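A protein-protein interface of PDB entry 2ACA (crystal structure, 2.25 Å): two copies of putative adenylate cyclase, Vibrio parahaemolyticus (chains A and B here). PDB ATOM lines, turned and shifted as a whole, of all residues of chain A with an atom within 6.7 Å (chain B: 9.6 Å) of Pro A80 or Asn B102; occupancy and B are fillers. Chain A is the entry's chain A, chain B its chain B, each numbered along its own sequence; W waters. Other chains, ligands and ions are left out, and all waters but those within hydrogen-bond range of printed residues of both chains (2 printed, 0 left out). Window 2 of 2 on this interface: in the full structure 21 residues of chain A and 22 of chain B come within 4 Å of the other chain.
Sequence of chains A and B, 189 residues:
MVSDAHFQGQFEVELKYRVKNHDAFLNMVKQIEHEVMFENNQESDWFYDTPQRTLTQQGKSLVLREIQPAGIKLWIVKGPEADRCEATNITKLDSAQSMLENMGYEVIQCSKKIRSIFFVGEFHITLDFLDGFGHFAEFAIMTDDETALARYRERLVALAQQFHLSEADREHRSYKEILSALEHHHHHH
Among the printed residues, merely in contact across the chains: Val A77 with Met B99 (3.8 Å), Val A77 with Asn B102 (3.8 Å), Pro A80 with Asn B102 (3.7 Å) and Arg A84 with Asn B102 (3.6 Å).
Of the printed residues of chain B, Lys A60 touches Asn B102 (2.9 Å).
Printed residues of chain B within 4 Å of Val A77: Met B99 and Asn B102.
Lys A78 touches none of the printed residues of chain B.
Of chain B, only Asn B102 comes within 4 Å of Gly A79.
Pro A80 touches just one residue of chain B: Asn B102 (3.7 Å).
No residue of chain B comes within 4 Å of Glu A81.
Printed residues of chain B within 4 Å of Glu A86: Ser B98 (2.8 Å) and Met B99 (3.5 Å).
Ser B95 touches none of the printed residues of chain A.
Printed residues of chain A within 4 Å of Ser B98: Arg A84 and Glu A86.
Printed residues of chain A within 4 Å of Met B99: Val A77 and Glu A86.
Of chain A, only Lys A60, Val A77, Gly A79, Pro A80 and Arg A84 come within 4 Å of Asn B102.
The nearest residue of chain A that does not touch Asn B102 is Glu A86 (4.6 Å).
The nearest printed residue of chain B that does not touch Val A77 is Met B103 (4.2 Å).
The side-chain amino group of Lys A60 sits at hydrogen-bond distance from the backbone carbonyl oxygen of Asn B102.
O of Gly A79 sits close to OD1 of Asn B102 (3.0 Å).
The guanidinium group of Arg A84 is in hydrogen-bond range of the side-chain hydroxyl of Ser B98 (3.4 Å).
OG of Ser B98 sits close to OE1 of Glu A86, at 2.9 Å.
O of Glu A86 sits close to SD of Met B99, at 3.5 Å.
Water W2 bridges the side-chain carboxylate (OE2) of Glu A86 (2.6 Å) and the side-chain amide oxygen (OD1) of Asn B102 (3.0 Å).
Water W1 bridges the guanidinium group of Arg A84 (2.8 Å) and the backbone carbonyl oxygen of Ser B98 (3.4 Å).
Of the 14 printed residues of chain B, 3 touch a printed residue of chain A.
Printed residues of chain B that touch a printed residue of chain A: Ser B98, Met B99 and Asn B102.
Along chain B the printed residues that touch a printed residue of chain A span positions 98 to 102.
Of the 13 printed residues of chain A, 6 touch a printed residue of chain B.
Among the printed residues, no Asp or Glu carboxylate lies within 4 Å of a Lys or Arg side-chain nitrogen of the other chain.
N of Lys A60 lies within hydrogen-bond range of O of Leu A55 (2.8 Å).
N of Glu A86 sits at hydrogen-bond distance from O of Val A77 (2.9 Å).
N of Gly A79 is in hydrogen-bond range of O of Arg A84.
The side-chain carboxylate of Glu A81 lies within salt-bridge range of the guanidinium group of Arg A84, 3.7 Å away.
The guanidinium group (NH2) of Arg A84 lies within salt-bridge range of the side-chain carboxylate (OE2) of Glu A86, at 2.7 Å.
No position is printed for both chains.
Of the 9 pairs that touch across the chains among the printed residues, none has its exchanged pair printed and touching as well.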
ATOM      1  N   LEU A  55      14.126  -5.108  20.854  1.00  0.00           N
ATOM      2  CA  LEU A  55      13.716  -3.759  21.192  1.00  0.00           C
ATOM      3  C   LEU A  55      12.273  -3.483  20.738  1.00  0.00           C
ATOM      4  O   LEU A  55      11.495  -2.861  21.462  1.00  0.00           O
ATOM      5  CB  LEU A  55      14.673  -2.753  20.557  1.00  0.00           C
ATOM      6  CG  LEU A  55      16.090  -2.825  21.132  1.00  0.00           C
ATOM      7  CD1 LEU A  55      17.000  -1.889  20.369  1.00  0.00           C
ATOM      8  CD2 LEU A  55      16.054  -2.469  22.609  1.00  0.00           C
ATOM      9  N   GLN A  58       9.657  -4.995  22.980  1.00  0.00           N
ATOM     10  CA  GLN A  58       9.572  -4.307  24.255  1.00  0.00           C
ATOM     11  C   GLN A  58       9.066  -2.866  24.154  1.00  0.00           C
ATOM     12  O   GLN A  58       9.057  -2.139  25.145  1.00  0.00           O
ATOM     13  CB  GLN A  58      10.944  -4.342  24.941  1.00  0.00           C
ATOM     14  CG  GLN A  58      11.367  -5.749  25.325  1.00  0.00           C
ATOM     15  CD  GLN A  58      10.374  -6.394  26.283  1.00  0.00           C
ATOM     16  OE1 GLN A  58      10.254  -7.621  26.345  1.00  0.00           O
ATOM     17  NE2 GLN A  58       9.659  -5.563  27.042  1.00  0.00           N
ATOM     18  N   GLY A  59       8.648  -2.455  22.961  1.00  0.00           N
ATOM     19  CA  GLY A  59       8.136  -1.105  22.773  1.00  0.00           C
ATOM     20  C   GLY A  59       9.226  -0.052  22.770  1.00  0.00           C
ATOM     21  O   GLY A  59       9.043   1.060  23.252  1.00  0.00           O
ATOM     22  N   LYS A  60      10.375  -0.400  22.216  1.00  0.00           N
ATOM     23  CA  LYS A  60      11.484   0.537  22.176  1.00  0.00           C
ATOM     24  C   LYS A  60      12.015   0.699  20.761  1.00  0.00           C
ATOM     25  O   LYS A  60      11.840  -0.172  19.915  1.00  0.00           O
ATOM     26  CB  LYS A  60      12.607   0.045  23.092  1.00  0.00           C
ATOM     27  CG  LYS A  60      12.186  -0.168  24.525  1.00  0.00           C
ATOM     28  CD  LYS A  60      13.275  -0.885  25.322  1.00  0.00           C
ATOM     29  CE  LYS A  60      12.839  -1.141  26.761  1.00  0.00           C
ATOM     30  NZ  LYS A  60      13.881  -1.867  27.527  1.00  0.00           N
ATOM     31  N   VAL A  77      16.992   6.784  21.670  1.00  0.00           N
ATOM     32  CA  VAL A  77      16.239   5.628  22.135  1.00  0.00           C
ATOM     33  C   VAL A  77      14.892   6.112  22.685  1.00  0.00           C
ATOM     34  O   VAL A  77      14.843   6.936  23.603  1.00  0.00           O
ATOM     35  CB  VAL A  77      16.970   4.840  23.217  1.00  0.00           C
ATOM     36  CG1 VAL A  77      16.106   3.691  23.665  1.00  0.00           C
ATOM     37  CG2 VAL A  77      18.286   4.307  22.672  1.00  0.00           C
ATOM     38  N   LYS A  78      13.806   5.608  22.100  1.00  0.00           N
ATOM     39  CA  LYS A  78      12.459   5.978  22.513  1.00  0.00           C
ATOM     40  C   LYS A  78      11.773   4.812  23.196  1.00  0.00           C
ATOM     41  O   LYS A  78      12.010   3.652  22.842  1.00  0.00           O
ATOM     42  CB  LYS A  78      11.621   6.412  21.307  1.00  0.00           C
ATOM     43  CG  LYS A  78      12.004   7.755  20.706  1.00  0.00           C
ATOM     44  CD  LYS A  78      11.135   8.075  19.496  1.00  0.00           C
ATOM     45  CE  LYS A  78      11.446   9.443  18.902  1.00  0.00           C
ATOM     46  NZ  LYS A  78      11.043  10.558  19.804  1.00  0.00           N
ATOM     47  N   GLY A  79      10.911   5.131  24.164  1.00  0.00           N
ATOM     48  CA  GLY A  79      10.188   4.098  24.894  1.00  0.00           C
ATOM     49  C   GLY A  79      10.965   3.572  26.089  1.00  0.00           C
ATOM     50  O   GLY A  79      12.064   4.058  26.370  1.00  0.00           O
ATOM     51  N   PRO A  80      10.429   2.580  26.818  1.00  0.00           N
ATOM     52  CA  PRO A  80       9.131   1.947  26.559  1.00  0.00           C
ATOM     53  C   PRO A  80       7.952   2.851  26.914  1.00  0.00           C
ATOM     54  O   PRO A  80       6.902   2.782  26.283  1.00  0.00           O
ATOM     55  CB  PRO A  80       9.183   0.691  27.424  1.00  0.00           C
ATOM     56  CG  PRO A  80       9.991   1.138  28.597  1.00  0.00           C
ATOM     57  CD  PRO A  80      11.119   1.911  27.936  1.00  0.00           C
ATOM     58  N   GLU A  81       8.128   3.695  27.926  1.00  0.00           N
ATOM     59  CA  GLU A  81       7.068   4.609  28.334  1.00  0.00           C
ATOM     60  C   GLU A  81       6.674   5.491  27.149  1.00  0.00           C
ATOM     61  O   GLU A  81       7.531   6.009  26.433  1.00  0.00           O
ATOM     62  CB  GLU A  81       7.530   5.482  29.507  1.00  0.00           C
ATOM     63  CG  GLU A  81       7.786   4.718  30.798  1.00  0.00           C
ATOM     64  CD  GLU A  81       9.061   3.892  30.760  1.00  0.00           C
ATOM     65  OE1 GLU A  81       9.326   3.155  31.736  1.00  0.00           O
ATOM     66  OE2 GLU A  81       9.802   3.981  29.759  1.00  0.00           O
ATOM     67  N   ALA A  82       5.370   5.652  26.952  1.00  0.00           N
ATOM     68  CA  ALA A  82       4.833   6.452  25.857  1.00  0.00           C
ATOM     69  C   ALA A  82       5.554   7.775  25.603  1.00  0.00           C
ATOM     70  O   ALA A  82       5.771   8.156  24.451  1.00  0.00           O
ATOM     71  CB  ALA A  82       3.351   6.715  26.097  1.00  0.00           C
ATOM     72  N   ASP A  83       5.925   8.467  26.677  1.00  0.00           N
ATOM     73  CA  ASP A  83       6.591   9.762  26.571  1.00  0.00           C
ATOM     74  C   ASP A  83       8.084   9.773  26.903  1.00  0.00           C
ATOM     75  O   ASP A  83       8.649  10.838  27.162  1.00  0.00           O
ATOM     76  CB  ASP A  83       5.889  10.763  27.484  1.00  0.00           C
ATOM     77  CG  ASP A  83       5.828  10.285  28.921  1.00  0.00           C
ATOM     78  OD1 ASP A  83       5.096   9.309  29.189  1.00  0.00           O
ATOM     79  OD2 ASP A  83       6.521  10.872  29.778  1.00  0.00           O
ATOM     80  N   ARG A  84       8.728   8.613  26.900  1.00  0.00           N
ATOM     81  CA  ARG A  84      10.151   8.572  27.219  1.00  0.00           C
ATOM     82  C   ARG A  84      11.021   8.610  25.970  1.00  0.00           C
ATOM     83  O   ARG A  84      10.848   7.813  25.044  1.00  0.00           O
ATOM     84  CB  ARG A  84      10.485   7.318  28.043  1.00  0.00           C
ATOM     85  CG  ARG A  84      11.944   7.242  28.512  1.00  0.00           C
ATOM     86  CD  ARG A  84      12.234   5.932  29.243  1.00  0.00           C
ATOM     87  NE  ARG A  84      13.639   5.810  29.628  1.00  0.00           N
ATOM     88  CZ  ARG A  84      14.168   4.750  30.240  1.00  0.00           C
ATOM     89  NH1 ARG A  84      13.411   3.701  30.544  1.00  0.00           N
ATOM     90  NH2 ARG A  84      15.461   4.735  30.548  1.00  0.00           N
ATOM     91  N   GLU A  86      15.260   9.443  25.021  1.00  0.00           N
ATOM     92  CA  GLU A  86      16.590   9.858  25.419  1.00  0.00           C
ATOM     93  C   GLU A  86      17.486   9.970  24.196  1.00  0.00           C
ATOM     94  O   GLU A  86      17.317   9.251  23.212  1.00  0.00           O
ATOM     95  CB  GLU A  86      17.169   8.871  26.433  1.00  0.00           C
ATOM     96  CG  GLU A  86      16.293   8.718  27.665  1.00  0.00           C
ATOM     97  CD  GLU A  86      16.959   7.922  28.769  1.00  0.00           C
ATOM     98  OE1 GLU A  86      17.978   8.398  29.314  1.00  0.00           O
ATOM     99  OE2 GLU A  86      16.463   6.823  29.089  1.00  0.00           O
ATOM    100  N   TYR B  48      30.457  -1.821  30.093  1.00  0.00           N
ATOM    101  CA  TYR B  48      29.103  -2.387  30.016  1.00  0.00           C
ATOM    102  C   TYR B  48      29.041  -3.740  29.334  1.00  0.00           C
ATOM    103  O   TYR B  48      29.875  -4.068  28.490  1.00  0.00           O
ATOM    104  CB  TYR B  48      28.154  -1.456  29.243  1.00  0.00           C
ATOM    105  CG  TYR B  48      27.791  -0.172  29.952  1.00  0.00           C
ATOM    106  CD1 TYR B  48      28.677   0.902  29.991  1.00  0.00           C
ATOM    107  CD2 TYR B  48      26.555  -0.034  30.589  1.00  0.00           C
ATOM    108  CE1 TYR B  48      28.345   2.079  30.638  1.00  0.00           C
ATOM    109  CE2 TYR B  48      26.217   1.141  31.243  1.00  0.00           C
ATOM    110  CZ  TYR B  48      27.117   2.195  31.260  1.00  0.00           C
ATOM    111  OH  TYR B  48      26.771   3.375  31.878  1.00  0.00           O
ATOM    112  N   ASP B  94      25.303  11.036  30.791  1.00  0.00           N
ATOM    113  CA  ASP B  94      24.216  10.382  31.516  1.00  0.00           C
ATOM    114  C   ASP B  94      23.147   9.789  30.603  1.00  0.00           C
ATOM    115  O   ASP B  94      22.558   8.760  30.922  1.00  0.00           O
ATOM    116  CB  ASP B  94      23.564  11.362  32.490  1.00  0.00           C
ATOM    117  CG  ASP B  94      22.992  12.571  31.794  1.00  0.00           C
ATOM    118  OD1 ASP B  94      21.794  12.862  31.997  1.00  0.00           O
ATOM    119  OD2 ASP B  94      23.740  13.230  31.042  1.00  0.00           O
ATOM    120  N   SER B  95      22.877  10.444  29.477  1.00  0.00           N
ATOM    121  CA  SER B  95      21.885   9.928  28.537  1.00  0.00           C
ATOM    122  C   SER B  95      22.412   8.616  27.961  1.00  0.00           C
ATOM    123  O   SER B  95      21.698   7.626  27.902  1.00  0.00           O
ATOM    124  CB  SER B  95      21.642  10.933  27.414  1.00  0.00           C
ATOM    125  OG  SER B  95      21.090  12.132  27.925  1.00  0.00           O
ATOM    126  N   ALA B  96      23.675   8.613  27.547  1.00  0.00           N
ATOM    127  CA  ALA B  96      24.282   7.399  27.007  1.00  0.00           C
ATOM    128  C   ALA B  96      24.185   6.297  28.056  1.00  0.00           C
ATOM    129  O   ALA B  96      23.816   5.162  27.753  1.00  0.00           O
ATOM    130  CB  ALA B  96      25.745   7.657  26.648  1.00  0.00           C
ATOM    131  N   GLN B  97      24.498   6.632  29.306  1.00  0.00           N
ATOM    132  CA  GLN B  97      24.426   5.639  30.368  1.00  0.00           C
ATOM    133  C   GLN B  97      23.022   5.068  30.451  1.00  0.00           C
ATOM    134  O   GLN B  97      22.834   3.857  30.494  1.00  0.00           O
ATOM    135  CB  GLN B  97      24.826   6.254  31.714  1.00  0.00           C
ATOM    136  CG  GLN B  97      26.292   6.662  31.793  1.00  0.00           C
ATOM    137  CD  GLN B  97      26.650   7.394  33.086  1.00  0.00           C
ATOM    138  OE1 GLN B  97      27.821   7.659  33.355  1.00  0.00           O
ATOM    139  NE2 GLN B  97      25.645   7.726  33.882  1.00  0.00           N
ATOM    140  N   SER B  98      22.030   5.952  30.449  1.00  0.00           N
ATOM    141  CA  SER B  98      20.642   5.524  30.540  1.00  0.00           C
ATOM    142  C   SER B  98      20.161   4.771  29.298  1.00  0.00           C
ATOM    143  O   SER B  98      19.326   3.871  29.390  1.00  0.00           O
ATOM    144  CB  SER B  98      19.739   6.731  30.795  1.00  0.00           C
ATOM    145  OG  SER B  98      18.455   6.299  31.197  1.00  0.00           O
ATOM    146  N   MET B  99      20.674   5.135  28.131  1.00  0.00           N
ATOM    147  CA  MET B  99      20.260   4.432  26.920  1.00  0.00           C
ATOM    148  C   MET B  99      20.809   2.996  26.892  1.00  0.00           C
ATOM    149  O   MET B  99      20.091   2.065  26.532  1.00  0.00           O
ATOM    150  CB  MET B  99      20.695   5.214  25.670  1.00  0.00           C
ATOM    151  CG  MET B  99      19.870   6.475  25.432  1.00  0.00           C
ATOM    152  SD  MET B  99      20.278   7.383  23.758  1.00  0.00           S
ATOM    153  CE  MET B  99      21.837   8.349  24.366  1.00  0.00           C
ATOM    154  N   LEU B 100      22.073   2.807  27.270  1.00  0.00           N
ATOM    155  CA  LEU B 100      22.644   1.449  27.296  1.00  0.00           C
ATOM    156  C   LEU B 100      21.875   0.586  28.291  1.00  0.00           C
ATOM    157  O   LEU B 100      21.698  -0.617  28.097  1.00  0.00           O
ATOM    158  CB  LEU B 100      24.124   1.480  27.687  1.00  0.00           C
ATOM    159  CG  LEU B 100      25.095   2.091  26.668  1.00  0.00           C
ATOM    160  CD1 LEU B 100      26.541   1.885  27.139  1.00  0.00           C
ATOM    161  CD2 LEU B 100      24.882   1.441  25.313  1.00  0.00           C
ATOM    162  N   GLU B 101      21.417   1.214  29.365  1.00  0.00           N
ATOM    163  CA  GLU B 101      20.640   0.526  30.401  1.00  0.00           C
ATOM    164  C   GLU B 101      19.311   0.073  29.793  1.00  0.00           C
ATOM    165  O   GLU B 101      18.870  -1.066  29.965  1.00  0.00           O
ATOM    166  CB  GLU B 101      20.352   1.497  31.546  1.00  0.00           C
ATOM    167  CG  GLU B 101      20.356   0.894  32.932  1.00  0.00           C
ATOM    168  CD  GLU B 101      21.728   0.944  33.571  1.00  0.00           C
ATOM    169  OE1 GLU B 101      22.630   0.217  33.109  1.00  0.00           O
ATOM    170  OE2 GLU B 101      21.905   1.724  34.533  1.00  0.00           O
ATOM    171  N   ASN B 102      18.672   0.984  29.073  1.00  0.00           N
ATOM    172  CA  ASN B 102      17.389   0.705  28.433  1.00  0.00           C
ATOM    173  C   ASN B 102      17.564  -0.391  27.384  1.00  0.00           C
ATOM    174  O   ASN B 102      16.661  -1.194  27.147  1.00  0.00           O
ATOM    175  CB  ASN B 102      16.865   1.990  27.780  1.00  0.00           C
ATOM    176  CG  ASN B 102      15.353   1.995  27.603  1.00  0.00           C
ATOM    177  OD1 ASN B 102      14.783   3.002  27.187  1.00  0.00           O
ATOM    178  ND2 ASN B 102      14.703   0.884  27.920  1.00  0.00           N
ATOM    179  N   MET B 103      18.739  -0.427  26.765  1.00  0.00           N
ATOM    180  CA  MET B 103      19.035  -1.417  25.734  1.00  0.00           C
ATOM    181  C   MET B 103      19.409  -2.792  26.292  1.00  0.00           C
ATOM    182  O   MET B 103      19.695  -3.718  25.532  1.00  0.00           O
ATOM    183  CB  MET B 103      20.145  -0.891  24.826  1.00  0.00           C
ATOM    184  CG  MET B 103      19.723   0.314  24.011  1.00  0.00           C
ATOM    185  SD  MET B 103      21.201   1.317  23.313  1.00  0.00           S
ATOM    186  CE  MET B 103      22.006  -0.028  22.174  1.00  0.00           C
ATOM    187  N   GLY B 104      19.414  -2.927  27.614  1.00  0.00           N
ATOM    188  CA  GLY B 104      19.718  -4.216  28.217  1.00  0.00           C
ATOM    189  C   GLY B 104      21.115  -4.432  28.785  1.00  0.00           C
ATOM    190  O   GLY B 104      21.472  -5.551  29.149  1.00  0.00           O
ATOM    191  N   TYR B 105      21.909  -3.375  28.868  1.00  0.00           N
ATOM    192  CA  TYR B 105      23.260  -3.503  29.396  1.00  0.00           C
ATOM    193  C   TYR B 105      23.301  -2.994  30.832  1.00  0.00           C
ATOM    194  O   TYR B 105      22.389  -2.289  31.282  1.00  0.00           O
ATOM    195  CB  TYR B 105      24.248  -2.685  28.556  1.00  0.00           C
ATOM    196  CG  TYR B 105      24.362  -3.126  27.110  1.00  0.00           C
ATOM    197  CD1 TYR B 105      25.141  -4.231  26.749  1.00  0.00           C
ATOM    198  CD2 TYR B 105      23.674  -2.444  26.100  1.00  0.00           C
ATOM    199  CE1 TYR B 105      25.231  -4.644  25.415  1.00  0.00           C
ATOM    200  CE2 TYR B 105      23.754  -2.849  24.767  1.00  0.00           C
ATOM    201  CZ  TYR B 105      24.533  -3.948  24.432  1.00  0.00           C
ATOM    202  OH  TYR B 105      24.598  -4.344  23.122  1.00  0.00           O
ATOM    203  N   GLU B 106      24.366  -3.355  31.536  1.00  0.00           N
ATOM    204  CA  GLU B 106      24.575  -2.927  32.908  1.00  0.00           C
ATOM    205  C   GLU B 106      26.068  -2.674  33.077  1.00  0.00           C
ATOM    206  O   GLU B 106      26.895  -3.188  32.315  1.00  0.00           O
ATOM    207  CB  GLU B 106      24.132  -4.018  33.894  1.00  0.00           C
ATOM    208  CG  GLU B 106      24.934  -5.307  33.774  1.00  0.00           C
ATOM    209  CD  GLU B 106      24.443  -6.410  34.696  1.00  0.00           C
ATOM    210  OE1 GLU B 106      23.230  -6.715  34.679  1.00  0.00           O
ATOM    211  OE2 GLU B 106      25.275  -6.983  35.432  1.00  0.00           O
HETATM  212  O   HOH W   1      17.236   3.047  31.949  1.00  0.00           O
HETATM  213  O   HOH W   2      16.508   5.394  26.932  1.00  0.00           O
